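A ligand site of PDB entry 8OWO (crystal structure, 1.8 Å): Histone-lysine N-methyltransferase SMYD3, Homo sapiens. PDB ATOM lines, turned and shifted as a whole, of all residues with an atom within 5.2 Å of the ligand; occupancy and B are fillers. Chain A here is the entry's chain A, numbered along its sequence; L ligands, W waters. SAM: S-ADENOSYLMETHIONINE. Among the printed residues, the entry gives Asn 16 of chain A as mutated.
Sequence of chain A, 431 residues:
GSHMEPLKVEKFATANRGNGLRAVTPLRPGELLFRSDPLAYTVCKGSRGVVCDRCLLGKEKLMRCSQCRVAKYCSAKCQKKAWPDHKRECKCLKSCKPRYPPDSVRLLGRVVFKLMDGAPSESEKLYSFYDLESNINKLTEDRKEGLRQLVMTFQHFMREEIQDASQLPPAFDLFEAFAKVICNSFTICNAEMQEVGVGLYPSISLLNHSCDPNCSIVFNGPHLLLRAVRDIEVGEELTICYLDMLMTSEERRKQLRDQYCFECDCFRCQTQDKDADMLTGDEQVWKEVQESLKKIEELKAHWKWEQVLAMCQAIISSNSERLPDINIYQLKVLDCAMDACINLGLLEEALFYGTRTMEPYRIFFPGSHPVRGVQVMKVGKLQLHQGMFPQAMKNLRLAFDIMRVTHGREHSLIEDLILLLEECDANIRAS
Water W5 lies within hydrogen-bond range of an oxygen (OXT) of the ligand (2.7 Å) and the side-chain carboxylate (OE1) of Glu 133 (2.8 Å). Water W4 lies within hydrogen-bond range of O of Cys 261 (2.6 Å), O2' of the ligand (2.8 Å) and OD1 of Asn 135 (3.0 Å). Water W1 lies within hydrogen-bond range of a nitrogen (N) of the ligand (2.8 Å), the side-chain carboxylate (OE1) of Glu 133 (3.0 Å) and the backbone carbonyl oxygen (O) of Arg 17 (3.5 Å). Water W6 lies within hydrogen-bond range of N1 of the ligand and O of Glu 263.
O of Tyr 260 sits at hydrogen-bond distance from ND2 of Asn 135, at 3.4 Å. OH of Tyr 260 sits at hydrogen-bond distance from NE2 of Gln 259 (3.1 Å). O of Arg 17 lies within hydrogen-bond range of ND2 of Asn 208, at 3.4 Å. The side-chain amide nitrogen (ND2) of Asn 208 sits at hydrogen-bond distance from the backbone carbonyl oxygen (O) of Asn 19 (3.2 Å). The side-chain amide nitrogen of Asn 184 lies within hydrogen-bond range of the side-chain sulfur of Cys 183 (3.4 Å). N of Asn 135 sits at hydrogen-bond distance from OE2 of Glu 133 (2.9 Å). The side-chain amide nitrogen (ND2) of Asn 135 lies within hydrogen-bond range of the side-chain sulfur (SG) of Cys 183, 3.7 Å away. O of Leu 207 lies within hydrogen-bond range of OH of Tyr 242.
An oxygen (O3') of the ligand sits at hydrogen-bond distance from the backbone carbonyl oxygen (O) of Tyr 260, at 2.6 Å. A nitrogen (N) of the ligand lies within hydrogen-bond range of the backbone carbonyl oxygen of Arg 17 (2.7 Å). The side-chain hydroxyl (OH) of Tyr 127 sits at hydrogen-bond distance from an oxygen (O) of the ligand. The backbone NH of Asn 19 sits at hydrogen-bond distance from an oxygen (OXT) of the ligand. O of Asn 19 lies within hydrogen-bond range of N of the ligand, at 2.8 Å. N of the ligand is in hydrogen-bond range of OD1 of Asn 208, 2.9 Å away. The backbone NH (N) of His 209 is in hydrogen-bond range of a nitrogen (N7) of the ligand (2.9 Å). O of His 209 is in hydrogen-bond range of N6 of the ligand, 2.9 Å away. O3' of the ligand is in hydrogen-bond range of ND2 of Asn 135.
The side-chain amide oxygen (OD1) of Asn 184 sits close to a sulfur (SD) of the ligand, at 3.4 Å. The backbone carbonyl oxygen (O) of Ser 205 sits close to a sulfur (SD) of the ligand, 3.4 Å away. The side-chain hydroxyl of Tyr 242 sits close to a sulfur (SD) of the ligand. Gly 18 touches the ligand (C to OXT, 3.8 Å). Glu 133 touches the ligand (CB to CE, 3.3 Å). Cys 183 touches the ligand (CB to O3', 3.8 Å). Leu 206 touches the ligand. O of Leu 207 touches CG of the ligand, at 3.6 Å. Phe 262 touches the ligand. Hydrophobic or aromatic side chains within 4 Å of the ligand: Tyr 127, His 209, Tyr 242, Tyr 260 and Phe 262. 16 residues have an atom within 4 Å of the ligand: Arg 17, Gly 18, Asn 19, Tyr 127, Glu 133, Asn 135, Cys 183, Asn 184, Ser 205, Leu 206, Leu 207, Asn 208, His 209, Tyr 242, Tyr 260 and Phe 262.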
ATOM      1  N   ASN A  16      22.561  -2.825   9.819  1.00  0.00           N
ATOM      2  CA  ASN A  16      23.097  -1.547   9.376  1.00  0.00           C
ATOM      3  C   ASN A  16      22.947  -1.275   7.883  1.00  0.00           C
ATOM      4  O   ASN A  16      23.656  -0.411   7.358  1.00  0.00           O
ATOM      5  CB  ASN A  16      24.603  -1.424   9.742  1.00  0.00           C
ATOM      6  CG  ASN A  16      25.453  -2.533   9.189  1.00  0.00           C
ATOM      7  OD1 ASN A  16      25.249  -3.018   8.068  1.00  0.00           O
ATOM      8  ND2 ASN A  16      26.448  -2.938   9.969  1.00  0.00           N
ATOM      9  N   ARG A  17      22.064  -1.937   7.191  1.00  0.00           N
ATOM     10  CA  ARG A  17      21.822  -1.572   5.802  1.00  0.00           C
ATOM     11  C   ARG A  17      20.332  -1.613   5.493  1.00  0.00           C
ATOM     12  O   ARG A  17      19.915  -2.034   4.411  1.00  0.00           O
ATOM     13  CB  ARG A  17      22.612  -2.449   4.844  1.00  0.00           C
ATOM     14  CG  ARG A  17      22.815  -3.865   5.264  1.00  0.00           C
ATOM     15  CD  ARG A  17      24.028  -4.428   4.559  1.00  0.00           C
ATOM     16  NE  ARG A  17      23.982  -5.881   4.419  1.00  0.00           N
ATOM     17  CZ  ARG A  17      24.998  -6.605   3.971  1.00  0.00           C
ATOM     18  NH1 ARG A  17      26.150  -6.051   3.635  1.00  0.00           N
ATOM     19  NH2 ARG A  17      24.850  -7.921   3.851  1.00  0.00           N
ATOM     20  N   GLY A  18      19.515  -1.166   6.443  1.00  0.00           N
ATOM     21  CA  GLY A  18      18.094  -1.063   6.203  1.00  0.00           C
ATOM     22  C   GLY A  18      17.439  -2.422   6.163  1.00  0.00           C
ATOM     23  O   GLY A  18      17.882  -3.393   6.796  1.00  0.00           O
ATOM     24  N   ASN A  19      16.353  -2.502   5.377  1.00  0.00           N
ATOM     25  CA  ASN A  19      15.698  -3.770   5.151  1.00  0.00           C
ATOM     26  C   ASN A  19      16.496  -4.597   4.153  1.00  0.00           C
ATOM     27  O   ASN A  19      17.273  -4.062   3.339  1.00  0.00           O
ATOM     28  CB  ASN A  19      14.285  -3.565   4.622  1.00  0.00           C
ATOM     29  CG  ASN A  19      13.422  -2.867   5.613  1.00  0.00           C
ATOM     30  OD1 ASN A  19      13.444  -3.217   6.806  1.00  0.00           O
ATOM     31  ND2 ASN A  19      12.744  -1.843   5.180  1.00  0.00           N
ATOM     32  N   GLY A  20      16.284  -5.901   4.229  1.00  0.00           N
ATOM     33  CA  GLY A  20      16.975  -6.839   3.359  1.00  0.00           C
ATOM     34  C   GLY A  20      16.128  -8.072   3.168  1.00  0.00           C
ATOM     35  O   GLY A  20      15.008  -8.165   3.654  1.00  0.00           O
ATOM     36  N   TYR A 127       7.355  -6.036  -0.843  1.00  0.00           N
ATOM     37  CA  TYR A 127       7.821  -4.667  -0.610  1.00  0.00           C
ATOM     38  C   TYR A 127       7.266  -3.819  -1.725  1.00  0.00           C
ATOM     39  O   TYR A 127       7.274  -4.247  -2.881  1.00  0.00           O
ATOM     40  CB  TYR A 127       9.360  -4.630  -0.624  1.00  0.00           C
ATOM     41  CG  TYR A 127      10.154  -3.593   0.169  1.00  0.00           C
ATOM     42  CD1 TYR A 127       9.960  -3.403   1.533  1.00  0.00           C
ATOM     43  CD2 TYR A 127      11.224  -2.928  -0.427  1.00  0.00           C
ATOM     44  CE1 TYR A 127      10.737  -2.533   2.240  1.00  0.00           C
ATOM     45  CE2 TYR A 127      12.007  -2.061   0.287  1.00  0.00           C
ATOM     46  CZ  TYR A 127      11.760  -1.862   1.617  1.00  0.00           C
ATOM     47  OH  TYR A 127      12.567  -1.030   2.350  1.00  0.00           O
ATOM     48  N   ASP A 131       7.289   1.593   0.181  1.00  0.00           N
ATOM     49  CA  ASP A 131       8.266   1.156   1.150  1.00  0.00           C
ATOM     50  C   ASP A 131       9.702   1.463   0.732  1.00  0.00           C
ATOM     51  O   ASP A 131      10.580   1.417   1.586  1.00  0.00           O
ATOM     52  CB  ASP A 131       8.208  -0.362   1.381  1.00  0.00           C
ATOM     53  CG  ASP A 131       6.887  -0.833   1.929  1.00  0.00           C
ATOM     54  OD1 ASP A 131       6.293  -0.129   2.777  1.00  0.00           O
ATOM     55  OD2 ASP A 131       6.484  -1.956   1.504  1.00  0.00           O
ATOM     56  N   LEU A 132       9.944   1.763  -0.541  1.00  0.00           N
ATOM     57  CA  LEU A 132      11.315   1.817  -1.030  1.00  0.00           C
ATOM     58  C   LEU A 132      12.142   2.843  -0.274  1.00  0.00           C
ATOM     59  O   LEU A 132      11.650   3.905   0.143  1.00  0.00           O
ATOM     60  CB  LEU A 132      11.350   2.134  -2.525  1.00  0.00           C
ATOM     61  CG  LEU A 132      10.770   1.110  -3.477  1.00  0.00           C
ATOM     62  CD1 LEU A 132      10.759   1.642  -4.906  1.00  0.00           C
ATOM     63  CD2 LEU A 132      11.579  -0.209  -3.345  1.00  0.00           C
ATOM     64  N   GLU A 133      13.430   2.546  -0.172  1.00  0.00           N
ATOM     65  CA  GLU A 133      14.407   3.466   0.407  1.00  0.00           C
ATOM     66  C   GLU A 133      14.628   4.657  -0.504  1.00  0.00           C
ATOM     67  O   GLU A 133      14.788   4.511  -1.727  1.00  0.00           O
ATOM     68  CB  GLU A 133      15.719   2.725   0.636  1.00  0.00           C
ATOM     69  CG  GLU A 133      16.832   3.579   1.129  1.00  0.00           C
ATOM     70  CD  GLU A 133      16.611   4.018   2.544  1.00  0.00           C
ATOM     71  OE1 GLU A 133      16.743   3.162   3.463  1.00  0.00           O
ATOM     72  OE2 GLU A 133      16.280   5.211   2.721  1.00  0.00           O
ATOM     73  N   ASN A 135      16.833   7.335   0.753  1.00  0.00           N
ATOM     74  CA  ASN A 135      18.084   7.934   1.219  1.00  0.00           C
ATOM     75  C   ASN A 135      18.032   9.450   1.292  1.00  0.00           C
ATOM     76  O   ASN A 135      19.055  10.116   1.103  1.00  0.00           O
ATOM     77  CB  ASN A 135      19.254   7.511   0.350  1.00  0.00           C
ATOM     78  CG  ASN A 135      19.640   6.111   0.610  1.00  0.00           C
ATOM     79  OD1 ASN A 135      19.873   5.761   1.754  1.00  0.00           O
ATOM     80  ND2 ASN A 135      19.657   5.290  -0.422  1.00  0.00           N
ATOM     81  N   CYS A 183      17.942   5.042  -6.493  1.00  0.00           N
ATOM     82  CA  CYS A 183      18.603   3.935  -5.812  1.00  0.00           C
ATOM     83  C   CYS A 183      17.826   2.628  -5.873  1.00  0.00           C
ATOM     84  O   CYS A 183      18.215   1.659  -5.234  1.00  0.00           O
ATOM     85  CB  CYS A 183      18.916   4.316  -4.365  1.00  0.00           C
ATOM     86  SG  CYS A 183      17.494   4.629  -3.321  1.00  0.00           S
ATOM     87  N   ASN A 184      16.779   2.543  -6.699  1.00  0.00           N
ATOM     88  CA  ASN A 184      16.038   1.290  -6.822  1.00  0.00           C
ATOM     89  C   ASN A 184      15.716   0.920  -8.270  1.00  0.00           C
ATOM     90  O   ASN A 184      14.935  -0.019  -8.487  1.00  0.00           O
ATOM     91  CB  ASN A 184      14.736   1.339  -6.024  1.00  0.00           C
ATOM     92  CG  ASN A 184      14.973   1.392  -4.517  1.00  0.00           C
ATOM     93  OD1 ASN A 184      15.345   0.380  -3.899  1.00  0.00           O
ATOM     94  ND2 ASN A 184      14.808   2.582  -3.928  1.00  0.00           N
ATOM     95  N   SER A 205      13.896  -5.102  -4.924  1.00  0.00           N
ATOM     96  CA  SER A 205      14.651  -4.023  -4.308  1.00  0.00           C
ATOM     97  C   SER A 205      14.980  -4.275  -2.838  1.00  0.00           C
ATOM     98  O   SER A 205      15.797  -3.537  -2.294  1.00  0.00           O
ATOM     99  CB  SER A 205      13.877  -2.721  -4.452  1.00  0.00           C
ATOM    100  OG  SER A 205      14.089  -2.236  -5.761  1.00  0.00           O
ATOM    101  N   LEU A 206      14.427  -5.307  -2.194  1.00  0.00           N
ATOM    102  CA  LEU A 206      14.892  -5.617  -0.850  1.00  0.00           C
ATOM    103  C   LEU A 206      16.339  -6.099  -0.814  1.00  0.00           C
ATOM    104  O   LEU A 206      16.972  -6.016   0.230  1.00  0.00           O
ATOM    105  CB  LEU A 206      14.018  -6.688  -0.193  1.00  0.00           C
ATOM    106  CG  LEU A 206      12.741  -6.173   0.445  1.00  0.00           C
ATOM    107  CD1 LEU A 206      11.827  -7.387   0.789  1.00  0.00           C
ATOM    108  CD2 LEU A 206      13.037  -5.383   1.668  1.00  0.00           C
ATOM    109  N   LEU A 207      16.866  -6.605  -1.920  1.00  0.00           N
ATOM    110  CA  LEU A 207      18.200  -7.191  -1.893  1.00  0.00           C
ATOM    111  C   LEU A 207      19.269  -6.107  -1.749  1.00  0.00           C
ATOM    112  O   LEU A 207      19.377  -5.211  -2.592  1.00  0.00           O
ATOM    113  CB  LEU A 207      18.464  -8.002  -3.162  1.00  0.00           C
ATOM    114  CG  LEU A 207      17.638  -9.274  -3.348  1.00  0.00           C
ATOM    115  CD1 LEU A 207      17.393  -9.561  -4.810  1.00  0.00           C
ATOM    116  CD2 LEU A 207      18.354 -10.449  -2.723  1.00  0.00           C
ATOM    117  N   ASN A 208      20.077  -6.200  -0.695  1.00  0.00           N
ATOM    118  CA  ASN A 208      21.248  -5.364  -0.585  1.00  0.00           C
ATOM    119  C   ASN A 208      22.373  -5.846  -1.502  1.00  0.00           C
ATOM    120  O   ASN A 208      22.359  -6.935  -2.064  1.00  0.00           O
ATOM    121  CB  ASN A 208      21.669  -5.317   0.867  1.00  0.00           C
ATOM    122  CG  ASN A 208      20.723  -4.477   1.673  1.00  0.00           C
ATOM    123  OD1 ASN A 208      20.398  -3.358   1.270  1.00  0.00           O
ATOM    124  ND2 ASN A 208      20.242  -5.006   2.786  1.00  0.00           N
ATOM    125  N   HIS A 209      23.364  -4.964  -1.652  1.00  0.00           N
ATOM    126  CA  HIS A 209      24.511  -5.148  -2.538  1.00  0.00           C
ATOM    127  C   HIS A 209      25.684  -5.873  -1.897  1.00  0.00           C
ATOM    128  O   HIS A 209      26.031  -5.636  -0.729  1.00  0.00           O
ATOM    129  CB  HIS A 209      25.011  -3.780  -2.989  1.00  0.00           C
ATOM    130  CG  HIS A 209      26.352  -3.815  -3.628  1.00  0.00           C
ATOM    131  ND1 HIS A 209      26.529  -4.055  -4.973  1.00  0.00           N
ATOM    132  CD2 HIS A 209      27.582  -3.692  -3.096  1.00  0.00           C
ATOM    133  CE1 HIS A 209      27.824  -4.043  -5.240  1.00  0.00           C
ATOM    134  NE2 HIS A 209      28.485  -3.849  -4.122  1.00  0.00           N
ATOM    135  N   SER A 210      26.379  -6.674  -2.700  1.00  0.00           N
ATOM    136  CA  SER A 210      27.697  -7.182  -2.356  1.00  0.00           C
ATOM    137  C   SER A 210      28.564  -7.243  -3.603  1.00  0.00           C
ATOM    138  O   SER A 210      28.074  -7.578  -4.690  1.00  0.00           O
ATOM    139  CB  SER A 210      27.625  -8.578  -1.731  1.00  0.00           C
ATOM    140  OG  SER A 210      28.924  -9.107  -1.627  1.00  0.00           O
ATOM    141  N   TYR A 242      25.136  -4.858  -7.446  1.00  0.00           N
ATOM    142  CA  TYR A 242      24.450  -3.812  -8.194  1.00  0.00           C
ATOM    143  C   TYR A 242      25.237  -3.356  -9.421  1.00  0.00           C
ATOM    144  O   TYR A 242      24.682  -2.631 -10.266  1.00  0.00           O
ATOM    145  CB  TYR A 242      24.233  -2.577  -7.331  1.00  0.00           C
ATOM    146  CG  TYR A 242      23.310  -2.705  -6.144  1.00  0.00           C
ATOM    147  CD1 TYR A 242      22.637  -3.896  -5.863  1.00  0.00           C
ATOM    148  CD2 TYR A 242      23.088  -1.615  -5.307  1.00  0.00           C
ATOM    149  CE1 TYR A 242      21.769  -3.984  -4.779  1.00  0.00           C
ATOM    150  CE2 TYR A 242      22.233  -1.701  -4.219  1.00  0.00           C
ATOM    151  CZ  TYR A 242      21.577  -2.887  -3.951  1.00  0.00           C
ATOM    152  OH  TYR A 242      20.714  -2.951  -2.845  1.00  0.00           O
ATOM    153  N   GLN A 259      25.027   6.993  -6.402  1.00  0.00           N
ATOM    154  CA  GLN A 259      23.709   6.456  -6.732  1.00  0.00           C
ATOM    155  C   GLN A 259      23.006   5.848  -5.529  1.00  0.00           C
ATOM    156  O   GLN A 259      21.778   5.977  -5.396  1.00  0.00           O
ATOM    157  CB  GLN A 259      23.848   5.409  -7.862  1.00  0.00           C
ATOM    158  CG  GLN A 259      22.522   4.864  -8.362  1.00  0.00           C
ATOM    159  CD  GLN A 259      22.655   3.867  -9.505  1.00  0.00           C
ATOM    160  OE1 GLN A 259      23.735   3.645 -10.059  1.00  0.00           O
ATOM    161  NE2 GLN A 259      21.538   3.249  -9.843  1.00  0.00           N
ATOM    162  N   TYR A 260      23.756   5.206  -4.631  1.00  0.00           N
ATOM    163  CA  TYR A 260      23.137   4.429  -3.563  1.00  0.00           C
ATOM    164  C   TYR A 260      23.408   4.949  -2.167  1.00  0.00           C
ATOM    165  O   TYR A 260      22.884   4.366  -1.202  1.00  0.00           O
ATOM    166  CB  TYR A 260      23.575   2.969  -3.657  1.00  0.00           C
ATOM    167  CG  TYR A 260      23.139   2.307  -4.977  1.00  0.00           C
ATOM    168  CD1 TYR A 260      21.846   1.801  -5.125  1.00  0.00           C
ATOM    169  CD2 TYR A 260      24.020   2.194  -6.031  1.00  0.00           C
ATOM    170  CE1 TYR A 260      21.443   1.182  -6.307  1.00  0.00           C
ATOM    171  CE2 TYR A 260      23.610   1.605  -7.235  1.00  0.00           C
ATOM    172  CZ  TYR A 260      22.339   1.093  -7.349  1.00  0.00           C
ATOM    173  OH  TYR A 260      21.980   0.474  -8.527  1.00  0.00           O
ATOM    174  N   CYS A 261      24.203   5.996  -2.023  1.00  0.00           N
ATOM    175  CA  CYS A 261      24.495   6.594  -0.707  1.00  0.00           C
ATOM    176  C   CYS A 261      24.947   5.580   0.346  1.00  0.00           C
ATOM    177  O   CYS A 261      24.493   5.604   1.500  1.00  0.00           O
ATOM    178  CB  CYS A 261      23.272   7.370  -0.172  1.00  0.00           C
ATOM    179  SG  CYS A 261      22.797   8.784  -1.172  1.00  0.00           S
ATOM    180  N   PHE A 262      25.922   4.735   0.004  1.00  0.00           N
ATOM    181  CA  PHE A 262      26.588   3.967   1.058  1.00  0.00           C
ATOM    182  C   PHE A 262      28.032   3.674   0.701  1.00  0.00           C
ATOM    183  O   PHE A 262      28.455   3.790  -0.455  1.00  0.00           O
ATOM    184  CB  PHE A 262      25.832   2.673   1.391  1.00  0.00           C
ATOM    185  CG  PHE A 262      25.995   1.578   0.373  1.00  0.00           C
ATOM    186  CD1 PHE A 262      25.142   1.492  -0.732  1.00  0.00           C
ATOM    187  CD2 PHE A 262      26.967   0.602   0.532  1.00  0.00           C
ATOM    188  CE1 PHE A 262      25.292   0.473  -1.684  1.00  0.00           C
ATOM    189  CE2 PHE A 262      27.117  -0.418  -0.420  1.00  0.00           C
ATOM    190  CZ  PHE A 262      26.288  -0.492  -1.512  1.00  0.00           C
ATOM    191  N   GLU A 263      28.774   3.322   1.754  1.00  0.00           N
ATOM    192  CA  GLU A 263      30.184   2.980   1.692  1.00  0.00           C
ATOM    193  C   GLU A 263      30.291   1.467   1.847  1.00  0.00           C
ATOM    194  O   GLU A 263      29.686   0.916   2.757  1.00  0.00           O
ATOM    195  CB  GLU A 263      30.962   3.670   2.829  1.00  0.00           C
ATOM    196  CG  GLU A 263      30.484   5.081   3.152  1.00  0.00           C
ATOM    197  CD  GLU A 263      30.815   6.048   2.039  1.00  0.00           C
ATOM    198  OE1 GLU A 263      31.591   5.670   1.118  1.00  0.00           O
ATOM    199  OE2 GLU A 263      30.291   7.165   2.093  1.00  0.00           O
ATOM    200  N   CYS A 264      31.064   0.821   0.980  1.00  0.00           N
ATOM    201  CA  CYS A 264      31.130  -0.630   1.015  1.00  0.00           C
ATOM    202  C   CYS A 264      32.314  -1.086   1.842  1.00  0.00           C
ATOM    203  O   CYS A 264      33.454  -0.658   1.583  1.00  0.00           O
ATOM    204  CB  CYS A 264      31.220  -1.261  -0.364  1.00  0.00           C
ATOM    205  SG  CYS A 264      31.104  -3.095  -0.127  1.00  0.00           S
HETATM  206  N   SAM L   1      18.308  -1.712   2.293  1.00  0.00           N
HETATM  207  CA  SAM L   1      17.332  -1.304   1.278  1.00  0.00           C
HETATM  208  C   SAM L   1      15.989  -0.939   1.900  1.00  0.00           C
HETATM  209  O   SAM L   1      15.011  -0.720   1.183  1.00  0.00           O
HETATM  210  OXT SAM L   1      15.886  -0.828   3.125  1.00  0.00           O
HETATM  211  CB  SAM L   1      17.118  -2.394   0.232  1.00  0.00           C
HETATM  212  CG  SAM L   1      18.117  -2.311  -0.932  1.00  0.00           C
HETATM  213  SD  SAM L   1      17.821  -0.853  -2.000  1.00  0.00           S
HETATM  214  CE  SAM L   1      16.574   0.289  -1.357  1.00  0.00           C
HETATM  215  C5' SAM L   1      19.419   0.029  -2.040  1.00  0.00           C
HETATM  216  C4' SAM L   1      19.819   0.708  -0.737  1.00  0.00           C
HETATM  217  O4' SAM L   1      20.090  -0.228   0.304  1.00  0.00           O
HETATM  218  C3' SAM L   1      21.091   1.559  -0.871  1.00  0.00           C
HETATM  219  O3' SAM L   1      20.811   2.826  -1.471  1.00  0.00           O
HETATM  220  C2' SAM L   1      21.582   1.600   0.572  1.00  0.00           C
HETATM  221  O2' SAM L   1      20.753   2.469   1.300  1.00  0.00           O
HETATM  222  C1' SAM L   1      21.250   0.189   1.036  1.00  0.00           C
HETATM  223  N9  SAM L   1      22.307  -0.814   0.769  1.00  0.00           N
HETATM  224  C8  SAM L   1      22.313  -1.753  -0.227  1.00  0.00           C
HETATM  225  N7  SAM L   1      23.449  -2.500  -0.086  1.00  0.00           N
HETATM  226  C5  SAM L   1      24.147  -2.036   0.992  1.00  0.00           C
HETATM  227  C6  SAM L   1      25.360  -2.380   1.561  1.00  0.00           C
HETATM  228  N6  SAM L   1      26.140  -3.405   1.117  1.00  0.00           N
HETATM  229  N1  SAM L   1      25.768  -1.644   2.640  1.00  0.00           N
HETATM  230  C2  SAM L   1      25.012  -0.604   3.157  1.00  0.00           C
HETATM  231  N3  SAM L   1      23.817  -0.245   2.594  1.00  0.00           N
HETATM  232  C4  SAM L   1      23.419  -0.946   1.510  1.00  0.00           C
HETATM  233  O   HOH W   1      18.732   0.948   3.083  1.00  0.00           O
HETATM  234  O   HOH W   2      28.931  -4.114   1.979  1.00  0.00           O
HETATM  235  O   HOH W   3      23.141   2.005   4.198  1.00  0.00           O
HETATM  236  O   HOH W   4      22.450   4.361   2.444  1.00  0.00           O
HETATM  237  O   HOH W   5      14.746   1.382   4.204  1.00  0.00           O
HETATM  238  O   HOH W   6      28.385  -1.714   3.976  1.00  0.00           O
